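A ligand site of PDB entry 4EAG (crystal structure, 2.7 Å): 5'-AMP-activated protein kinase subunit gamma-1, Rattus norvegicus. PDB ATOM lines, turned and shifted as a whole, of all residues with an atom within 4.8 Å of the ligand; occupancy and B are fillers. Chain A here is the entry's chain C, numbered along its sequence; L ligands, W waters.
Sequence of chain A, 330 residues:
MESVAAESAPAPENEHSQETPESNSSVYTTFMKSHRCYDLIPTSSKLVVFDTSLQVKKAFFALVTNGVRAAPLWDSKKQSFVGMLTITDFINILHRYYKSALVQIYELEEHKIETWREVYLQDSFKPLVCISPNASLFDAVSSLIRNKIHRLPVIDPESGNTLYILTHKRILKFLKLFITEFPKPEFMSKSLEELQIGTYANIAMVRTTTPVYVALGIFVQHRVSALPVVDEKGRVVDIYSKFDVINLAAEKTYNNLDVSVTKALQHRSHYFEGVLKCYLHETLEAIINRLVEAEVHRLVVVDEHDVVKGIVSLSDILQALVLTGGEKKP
NZ of Lys 242 lies within hydrogen-bond range of OG1 of Thr 88 (2.9 Å). The backbone NH of Thr 86 lies within hydrogen-bond range of the side-chain carboxylate of Asp 89. The side-chain carboxylate of Asp 89 sits at hydrogen-bond distance from the side-chain amide nitrogen of Gln 122. N of Thr 88 sits close to OG1 of Thr 86 (3.5 Å). The backbone NH (N) of Gln 122 is in hydrogen-bond range of the backbone carbonyl oxygen (O) of Arg 117 (2.7 Å).
The backbone carbonyl oxygen (O) of Arg 151 sits at hydrogen-bond distance from a nitrogen (N3) of the ligand, 3.3 Å away. N of His 150 is in hydrogen-bond range of O8 of the ligand (3.0 Å). O of Val 129 lies within hydrogen-bond range of N3 of the ligand, at 2.8 Å. An oxygen (O5) of the ligand sits at hydrogen-bond distance from the side-chain hydroxyl (OG1) of Thr 88 (2.6 Å). The side-chain carboxylate (OD2) of Asp 89 is in hydrogen-bond range of an oxygen (O12) of the ligand. The guanidinium group of Arg 151 is in salt-bridge range of an oxygen (O3) of the ligand (2.9 Å). OG of Ser 225 sits at hydrogen-bond distance from O4 of the ligand, 3.4 Å away. The side-chain amide nitrogen (NE2) of Gln 122 lies within hydrogen-bond range of an oxygen (O13) of the ligand (3.4 Å). The backbone carbonyl oxygen (O) of Met 84 lies within hydrogen-bond range of an oxygen (O13) of the ligand (2.9 Å). The backbone NH (N) of Thr 88 is in hydrogen-bond range of an oxygen (O5) of the ligand, 2.8 Å away. O5 of the ligand is in hydrogen-bond range of OG1 of Thr 86 (2.8 Å). The backbone NH (N) of Val 129 lies within hydrogen-bond range of a nitrogen (N4) of the ligand, 2.8 Å away. A ring nitrogen (ND1) of His 150 is in hydrogen-bond range of an oxygen (O2) of the ligand.
Water W1 lies within hydrogen-bond range of O8 of the ligand (2.5 Å) and NE2 of His 150 (3.4 Å).
Residues that only touch the ligand: Pro 153 (3.4 Å), Ile 149 (3.4 Å), Leu 128 (3.5 Å), Pro 127 (3.6 Å), Ile 87 (3.6 Å), Phe 243 (3.7 Å) and Lys 126 (3.7 Å). Hydrophobic or aromatic side chains that line the ligand: Met 84, Ile 87, Leu 128, Val 129, Ile 149, His 150, Pro 153 and Phe 243. Of the 22 residues printed, 16 come within 4 Å of the ligand. Along chain A the residues within 4 Å of the ligand span positions 84 to 243.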
ATOM      1  N   ARG A  69      11.483   4.149  15.046  1.00  0.00           N
ATOM      2  CA  ARG A  69      10.622   3.342  14.185  1.00  0.00           C
ATOM      3  C   ARG A  69       9.206   3.145  14.773  1.00  0.00           C
ATOM      4  O   ARG A  69       8.325   2.637  14.093  1.00  0.00           O
ATOM      5  CB  ARG A  69      11.283   2.002  13.824  1.00  0.00           C
ATOM      6  CG  ARG A  69      12.460   2.083  12.799  1.00  0.00           C
ATOM      7  CD  ARG A  69      13.633   2.938  13.313  1.00  0.00           C
ATOM      8  NE  ARG A  69      14.685   3.196  12.338  1.00  0.00           N
ATOM      9  CZ  ARG A  69      14.759   4.293  11.568  1.00  0.00           C
ATOM     10  NH1 ARG A  69      13.828   5.230  11.644  1.00  0.00           N
ATOM     11  NH2 ARG A  69      15.765   4.441  10.715  1.00  0.00           N
ATOM     12  N   GLY A  83      -1.666   1.908  23.283  1.00  0.00           N
ATOM     13  CA  GLY A  83      -0.910   1.034  22.418  1.00  0.00           C
ATOM     14  C   GLY A  83       0.228   1.720  21.687  1.00  0.00           C
ATOM     15  O   GLY A  83       0.677   2.790  22.101  1.00  0.00           O
ATOM     16  N   MET A  84       0.674   1.101  20.600  1.00  0.00           N
ATOM     17  CA  MET A  84       1.836   1.565  19.827  1.00  0.00           C
ATOM     18  C   MET A  84       1.427   2.034  18.434  1.00  0.00           C
ATOM     19  O   MET A  84       0.542   1.435  17.814  1.00  0.00           O
ATOM     20  CB  MET A  84       2.821   0.420  19.641  1.00  0.00           C
ATOM     21  CG  MET A  84       3.486  -0.065  20.881  1.00  0.00           C
ATOM     22  SD  MET A  84       4.670   1.130  21.470  1.00  0.00           S
ATOM     23  CE  MET A  84       3.885   1.599  23.008  1.00  0.00           C
ATOM     24  N   THR A  86       3.106   1.685  15.023  1.00  0.00           N
ATOM     25  CA  THR A  86       4.212   0.990  14.380  1.00  0.00           C
ATOM     26  C   THR A  86       4.048   1.000  12.879  1.00  0.00           C
ATOM     27  O   THR A  86       3.015   1.403  12.366  1.00  0.00           O
ATOM     28  CB  THR A  86       4.346  -0.485  14.838  1.00  0.00           C
ATOM     29  OG1 THR A  86       3.244  -1.251  14.328  1.00  0.00           O
ATOM     30  CG2 THR A  86       4.374  -0.594  16.344  1.00  0.00           C
ATOM     31  N   ILE A  87       5.068   0.540  12.175  1.00  0.00           N
ATOM     32  CA  ILE A  87       5.041   0.509  10.734  1.00  0.00           C
ATOM     33  C   ILE A  87       3.891  -0.342  10.141  1.00  0.00           C
ATOM     34  O   ILE A  87       3.421  -0.061   9.057  1.00  0.00           O
ATOM     35  CB  ILE A  87       6.388   0.029  10.197  1.00  0.00           C
ATOM     36  CG1 ILE A  87       6.760   0.808   8.929  1.00  0.00           C
ATOM     37  CG2 ILE A  87       6.393  -1.505  10.071  1.00  0.00           C
ATOM     38  CD1 ILE A  87       5.815   0.567   7.764  1.00  0.00           C
ATOM     39  N   THR A  88       3.430  -1.370  10.863  1.00  0.00           N
ATOM     40  CA  THR A  88       2.289  -2.155  10.378  1.00  0.00           C
ATOM     41  C   THR A  88       1.009  -1.310  10.311  1.00  0.00           C
ATOM     42  O   THR A  88       0.217  -1.409   9.382  1.00  0.00           O
ATOM     43  CB  THR A  88       2.010  -3.357  11.257  1.00  0.00           C
ATOM     44  OG1 THR A  88       3.033  -4.339  11.054  1.00  0.00           O
ATOM     45  CG2 THR A  88       0.657  -3.953  10.920  1.00  0.00           C
ATOM     46  N   ASP A  89       0.814  -0.477  11.320  1.00  0.00           N
ATOM     47  CA  ASP A  89      -0.346   0.396  11.317  1.00  0.00           C
ATOM     48  C   ASP A  89      -0.393   1.316  10.082  1.00  0.00           C
ATOM     49  O   ASP A  89      -1.439   1.435   9.475  1.00  0.00           O
ATOM     50  CB  ASP A  89      -0.398   1.182  12.633  1.00  0.00           C
ATOM     51  CG  ASP A  89      -0.303   0.278  13.848  1.00  0.00           C
ATOM     52  OD1 ASP A  89       0.655   0.440  14.645  1.00  0.00           O
ATOM     53  OD2 ASP A  89      -1.178  -0.596  14.003  1.00  0.00           O
ATOM     54  N   ARG A 117      -7.289   4.149  14.367  1.00  0.00           N
ATOM     55  CA  ARG A 117      -7.329   3.085  15.367  1.00  0.00           C
ATOM     56  C   ARG A 117      -8.770   2.740  15.705  1.00  0.00           C
ATOM     57  O   ARG A 117      -9.076   1.613  16.072  1.00  0.00           O
ATOM     58  CB  ARG A 117      -6.629   3.519  16.658  1.00  0.00           C
ATOM     59  CG  ARG A 117      -5.184   3.926  16.553  1.00  0.00           C
ATOM     60  CD  ARG A 117      -4.575   4.084  17.957  1.00  0.00           C
ATOM     61  NE  ARG A 117      -4.895   2.971  18.865  1.00  0.00           N
ATOM     62  CZ  ARG A 117      -4.085   1.946  19.124  1.00  0.00           C
ATOM     63  NH1 ARG A 117      -2.887   1.855  18.585  1.00  0.00           N
ATOM     64  NH2 ARG A 117      -4.479   0.984  19.948  1.00  0.00           N
ATOM     65  N   GLN A 122      -9.235  -0.810  17.351  1.00  0.00           N
ATOM     66  CA  GLN A 122      -7.959  -1.363  17.764  1.00  0.00           C
ATOM     67  C   GLN A 122      -7.811  -1.399  19.271  1.00  0.00           C
ATOM     68  O   GLN A 122      -7.227  -2.331  19.785  1.00  0.00           O
ATOM     69  CB  GLN A 122      -6.815  -0.585  17.140  1.00  0.00           C
ATOM     70  CG  GLN A 122      -5.491  -1.340  17.145  1.00  0.00           C
ATOM     71  CD  GLN A 122      -4.423  -0.602  16.360  1.00  0.00           C
ATOM     72  OE1 GLN A 122      -4.726   0.112  15.386  1.00  0.00           O
ATOM     73  NE2 GLN A 122      -3.172  -0.767  16.763  1.00  0.00           N
ATOM     74  N   LYS A 126      -7.212  -5.200  20.111  1.00  0.00           N
ATOM     75  CA  LYS A 126      -5.829  -5.464  20.515  1.00  0.00           C
ATOM     76  C   LYS A 126      -5.351  -4.405  21.521  1.00  0.00           C
ATOM     77  O   LYS A 126      -4.617  -3.485  21.162  1.00  0.00           O
ATOM     78  CB  LYS A 126      -4.915  -5.492  19.277  1.00  0.00           C
ATOM     79  CG  LYS A 126      -3.409  -5.473  19.582  1.00  0.00           C
ATOM     80  CD  LYS A 126      -2.686  -6.661  18.958  1.00  0.00           C
ATOM     81  CE  LYS A 126      -1.648  -7.237  19.909  1.00  0.00           C
ATOM     82  NZ  LYS A 126      -2.280  -7.690  21.185  1.00  0.00           N
ATOM     83  N   PRO A 127      -5.782  -4.527  22.792  1.00  0.00           N
ATOM     84  CA  PRO A 127      -5.440  -3.530  23.806  1.00  0.00           C
ATOM     85  C   PRO A 127      -3.950  -3.530  24.087  1.00  0.00           C
ATOM     86  O   PRO A 127      -3.301  -4.540  23.806  1.00  0.00           O
ATOM     87  CB  PRO A 127      -6.196  -4.038  25.043  1.00  0.00           C
ATOM     88  CG  PRO A 127      -6.230  -5.493  24.853  1.00  0.00           C
ATOM     89  CD  PRO A 127      -6.464  -5.692  23.388  1.00  0.00           C
ATOM     90  N   LEU A 128      -3.431  -2.436  24.629  1.00  0.00           N
ATOM     91  CA  LEU A 128      -2.013  -2.330  24.989  1.00  0.00           C
ATOM     92  C   LEU A 128      -1.499  -3.518  25.806  1.00  0.00           C
ATOM     93  O   LEU A 128      -2.114  -3.929  26.790  1.00  0.00           O
ATOM     94  CB  LEU A 128      -1.737  -1.024  25.749  1.00  0.00           C
ATOM     95  CG  LEU A 128      -0.277  -0.831  26.187  1.00  0.00           C
ATOM     96  CD1 LEU A 128       0.554  -0.423  25.008  1.00  0.00           C
ATOM     97  CD2 LEU A 128      -0.151   0.197  27.256  1.00  0.00           C
ATOM     98  N   VAL A 129      -0.354  -4.052  25.401  1.00  0.00           N
ATOM     99  CA  VAL A 129       0.403  -5.017  26.206  1.00  0.00           C
ATOM    100  C   VAL A 129       1.620  -4.307  26.811  1.00  0.00           C
ATOM    101  O   VAL A 129       2.418  -3.703  26.102  1.00  0.00           O
ATOM    102  CB  VAL A 129       0.880  -6.168  25.337  1.00  0.00           C
ATOM    103  CG1 VAL A 129       1.542  -7.221  26.187  1.00  0.00           C
ATOM    104  CG2 VAL A 129      -0.290  -6.729  24.576  1.00  0.00           C
ATOM    105  N   LYS A 148       2.534 -11.995  19.913  1.00  0.00           N
ATOM    106  CA  LYS A 148       3.054 -11.712  18.592  1.00  0.00           C
ATOM    107  C   LYS A 148       3.263 -10.224  18.330  1.00  0.00           C
ATOM    108  O   LYS A 148       2.784  -9.696  17.334  1.00  0.00           O
ATOM    109  CB  LYS A 148       2.125 -12.301  17.537  1.00  0.00           C
ATOM    110  CG  LYS A 148       2.228 -13.816  17.379  1.00  0.00           C
ATOM    111  CD  LYS A 148       1.914 -14.247  15.933  1.00  0.00           C
ATOM    112  CE  LYS A 148       2.962 -13.756  14.943  1.00  0.00           C
ATOM    113  NZ  LYS A 148       2.698 -14.196  13.530  1.00  0.00           N
ATOM    114  N   ILE A 149       3.999  -9.542  19.202  1.00  0.00           N
ATOM    115  CA  ILE A 149       4.301  -8.115  19.012  1.00  0.00           C
ATOM    116  C   ILE A 149       5.811  -7.882  19.025  1.00  0.00           C
ATOM    117  O   ILE A 149       6.568  -8.749  19.435  1.00  0.00           O
ATOM    118  CB  ILE A 149       3.640  -7.257  20.090  1.00  0.00           C
ATOM    119  CG1 ILE A 149       3.842  -7.882  21.466  1.00  0.00           C
ATOM    120  CG2 ILE A 149       2.152  -7.117  19.810  1.00  0.00           C
ATOM    121  CD1 ILE A 149       2.975  -7.280  22.557  1.00  0.00           C
ATOM    122  N   HIS A 150       6.266  -6.720  18.569  1.00  0.00           N
ATOM    123  CA  HIS A 150       7.718  -6.474  18.544  1.00  0.00           C
ATOM    124  C   HIS A 150       8.156  -5.434  19.576  1.00  0.00           C
ATOM    125  O   HIS A 150       9.335  -5.391  19.940  1.00  0.00           O
ATOM    126  CB  HIS A 150       8.222  -6.109  17.132  1.00  0.00           C
ATOM    127  CG  HIS A 150       8.079  -7.227  16.141  1.00  0.00           C
ATOM    128  ND1 HIS A 150       8.378  -7.068  14.802  1.00  0.00           N
ATOM    129  CD2 HIS A 150       7.672  -8.511  16.284  1.00  0.00           C
ATOM    130  CE1 HIS A 150       8.149  -8.208  14.169  1.00  0.00           C
ATOM    131  NE2 HIS A 150       7.726  -9.095  15.036  1.00  0.00           N
ATOM    132  N   ARG A 151       7.223  -4.629  20.052  1.00  0.00           N
ATOM    133  CA  ARG A 151       7.517  -3.646  21.086  1.00  0.00           C
ATOM    134  C   ARG A 151       6.784  -3.924  22.413  1.00  0.00           C
ATOM    135  O   ARG A 151       5.636  -4.393  22.424  1.00  0.00           O
ATOM    136  CB  ARG A 151       7.205  -2.232  20.587  1.00  0.00           C
ATOM    137  CG  ARG A 151       7.741  -1.916  19.194  1.00  0.00           C
ATOM    138  CD  ARG A 151       9.110  -1.221  19.233  1.00  0.00           C
ATOM    139  NE  ARG A 151       9.621  -0.911  17.904  1.00  0.00           N
ATOM    140  CZ  ARG A 151      10.769  -0.256  17.678  1.00  0.00           C
ATOM    141  NH1 ARG A 151      11.507   0.153  18.700  1.00  0.00           N
ATOM    142  NH2 ARG A 151      11.169  -0.015  16.439  1.00  0.00           N
ATOM    143  N   LEU A 152       7.442  -3.627  23.515  1.00  0.00           N
ATOM    144  CA  LEU A 152       6.836  -3.866  24.815  1.00  0.00           C
ATOM    145  C   LEU A 152       7.205  -2.780  25.822  1.00  0.00           C
ATOM    146  O   LEU A 152       8.331  -2.724  26.314  1.00  0.00           O
ATOM    147  CB  LEU A 152       7.240  -5.233  25.339  1.00  0.00           C
ATOM    148  CG  LEU A 152       6.499  -5.614  26.604  1.00  0.00           C
ATOM    149  CD1 LEU A 152       5.077  -5.849  26.235  1.00  0.00           C
ATOM    150  CD2 LEU A 152       7.116  -6.849  27.212  1.00  0.00           C
ATOM    151  N   PRO A 153       6.253  -1.880  26.097  1.00  0.00           N
ATOM    152  CA  PRO A 153       6.335  -0.764  27.029  1.00  0.00           C
ATOM    153  C   PRO A 153       6.626  -1.197  28.439  1.00  0.00           C
ATOM    154  O   PRO A 153       5.886  -1.982  29.013  1.00  0.00           O
ATOM    155  CB  PRO A 153       4.933  -0.176  26.971  1.00  0.00           C
ATOM    156  CG  PRO A 153       4.450  -0.482  25.654  1.00  0.00           C
ATOM    157  CD  PRO A 153       4.986  -1.833  25.344  1.00  0.00           C
ATOM    158  N   SER A 225       7.776  -9.439   8.795  1.00  0.00           N
ATOM    159  CA  SER A 225       8.311  -8.116   8.626  1.00  0.00           C
ATOM    160  C   SER A 225       8.984  -7.929   7.264  1.00  0.00           C
ATOM    161  O   SER A 225       8.698  -6.975   6.562  1.00  0.00           O
ATOM    162  CB  SER A 225       9.246  -7.727   9.793  1.00  0.00           C
ATOM    163  OG  SER A 225       8.560  -6.898  10.735  1.00  0.00           O
ATOM    164  N   LYS A 242       8.537  -3.714   5.219  1.00  0.00           N
ATOM    165  CA  LYS A 242       7.279  -2.975   5.310  1.00  0.00           C
ATOM    166  C   LYS A 242       7.585  -1.521   5.196  1.00  0.00           C
ATOM    167  O   LYS A 242       6.854  -0.754   4.564  1.00  0.00           O
ATOM    168  CB  LYS A 242       6.594  -3.243   6.646  1.00  0.00           C
ATOM    169  CG  LYS A 242       5.717  -4.509   6.722  1.00  0.00           C
ATOM    170  CD  LYS A 242       5.422  -4.876   8.188  1.00  0.00           C
ATOM    171  CE  LYS A 242       4.232  -5.808   8.326  1.00  0.00           C
ATOM    172  NZ  LYS A 242       4.208  -6.565   9.636  1.00  0.00           N
ATOM    173  N   PHE A 243       8.694  -1.138   5.792  1.00  0.00           N
ATOM    174  CA  PHE A 243       9.161   0.229   5.751  1.00  0.00           C
ATOM    175  C   PHE A 243       9.307   0.681   4.333  1.00  0.00           C
ATOM    176  O   PHE A 243       8.840   1.746   3.976  1.00  0.00           O
ATOM    177  CB  PHE A 243      10.487   0.367   6.487  1.00  0.00           C
ATOM    178  CG  PHE A 243      10.347   0.145   7.947  1.00  0.00           C
ATOM    179  CD1 PHE A 243      10.412  -1.134   8.476  1.00  0.00           C
ATOM    180  CD2 PHE A 243      10.111   1.214   8.805  1.00  0.00           C
ATOM    181  CE1 PHE A 243      10.252  -1.345   9.831  1.00  0.00           C
ATOM    182  CE2 PHE A 243       9.959   1.008  10.150  1.00  0.00           C
ATOM    183  CZ  PHE A 243      10.034  -0.267  10.669  1.00  0.00           C
HETATM  184  P1  LIG L   1       8.156  -2.927  14.593  1.00  0.00           P
HETATM  185  O1  LIG L   1       8.920  -1.926  13.738  1.00  0.00           O
HETATM  186  O2  LIG L   1       8.386  -4.390  14.263  1.00  0.00           O
HETATM  187  O3  LIG L   1       8.164  -2.564  16.059  1.00  0.00           O
HETATM  188  P2  LIG L   1       5.870  -3.824  13.270  1.00  0.00           P
HETATM  189  O4  LIG L   1       6.883  -4.482  12.353  1.00  0.00           O
HETATM  190  O5  LIG L   1       4.639  -3.112  12.745  1.00  0.00           O
HETATM  191  O6  LIG L   1       6.599  -2.786  14.249  1.00  0.00           O
HETATM  192  P3  LIG L   1       4.771  -4.674  15.756  1.00  0.00           P
HETATM  193  O7  LIG L   1       5.609  -3.667  16.508  1.00  0.00           O
HETATM  194  O8  LIG L   1       4.424  -6.018  16.357  1.00  0.00           O
HETATM  195  O9  LIG L   1       5.399  -4.962  14.311  1.00  0.00           O
HETATM  196  O10 LIG L   1       3.365  -4.047  15.345  1.00  0.00           O
HETATM  197  C1  LIG L   1       2.373  -4.961  14.925  1.00  0.00           C
HETATM  198  C2  LIG L   1       1.027  -4.512  15.429  1.00  0.00           C
HETATM  199  O11 LIG L   1       1.045  -4.694  16.842  1.00  0.00           O
HETATM  200  C3  LIG L   1       0.728  -3.049  15.177  1.00  0.00           C
HETATM  201  O12 LIG L   1      -0.663  -2.942  14.892  1.00  0.00           O
HETATM  202  C4  LIG L   1       0.996  -2.373  16.502  1.00  0.00           C
HETATM  203  O13 LIG L   1       0.161  -1.217  16.652  1.00  0.00           O
HETATM  204  C5  LIG L   1       0.665  -3.485  17.493  1.00  0.00           C
HETATM  205  N1  LIG L   1       1.451  -3.423  18.756  1.00  0.00           N
HETATM  206  C6  LIG L   1       2.783  -3.322  18.881  1.00  0.00           C
HETATM  207  N2  LIG L   1       3.157  -3.287  20.184  1.00  0.00           N
HETATM  208  C7  LIG L   1       2.052  -3.377  20.937  1.00  0.00           C
HETATM  209  C8  LIG L   1       1.739  -3.398  22.382  1.00  0.00           C
HETATM  210  N3  LIG L   1       2.700  -3.318  23.340  1.00  0.00           N
HETATM  211  N4  LIG L   1       0.450  -3.497  22.735  1.00  0.00           N
HETATM  212  C9  LIG L   1      -0.517  -3.567  21.807  1.00  0.00           C
HETATM  213  N5  LIG L   1      -0.319  -3.548  20.476  1.00  0.00           N
HETATM  214  C10 LIG L   1       0.926  -3.454  19.988  1.00  0.00           C
HETATM  215  O   HOH W   1       4.620  -7.761  14.603  1.00  0.00           O
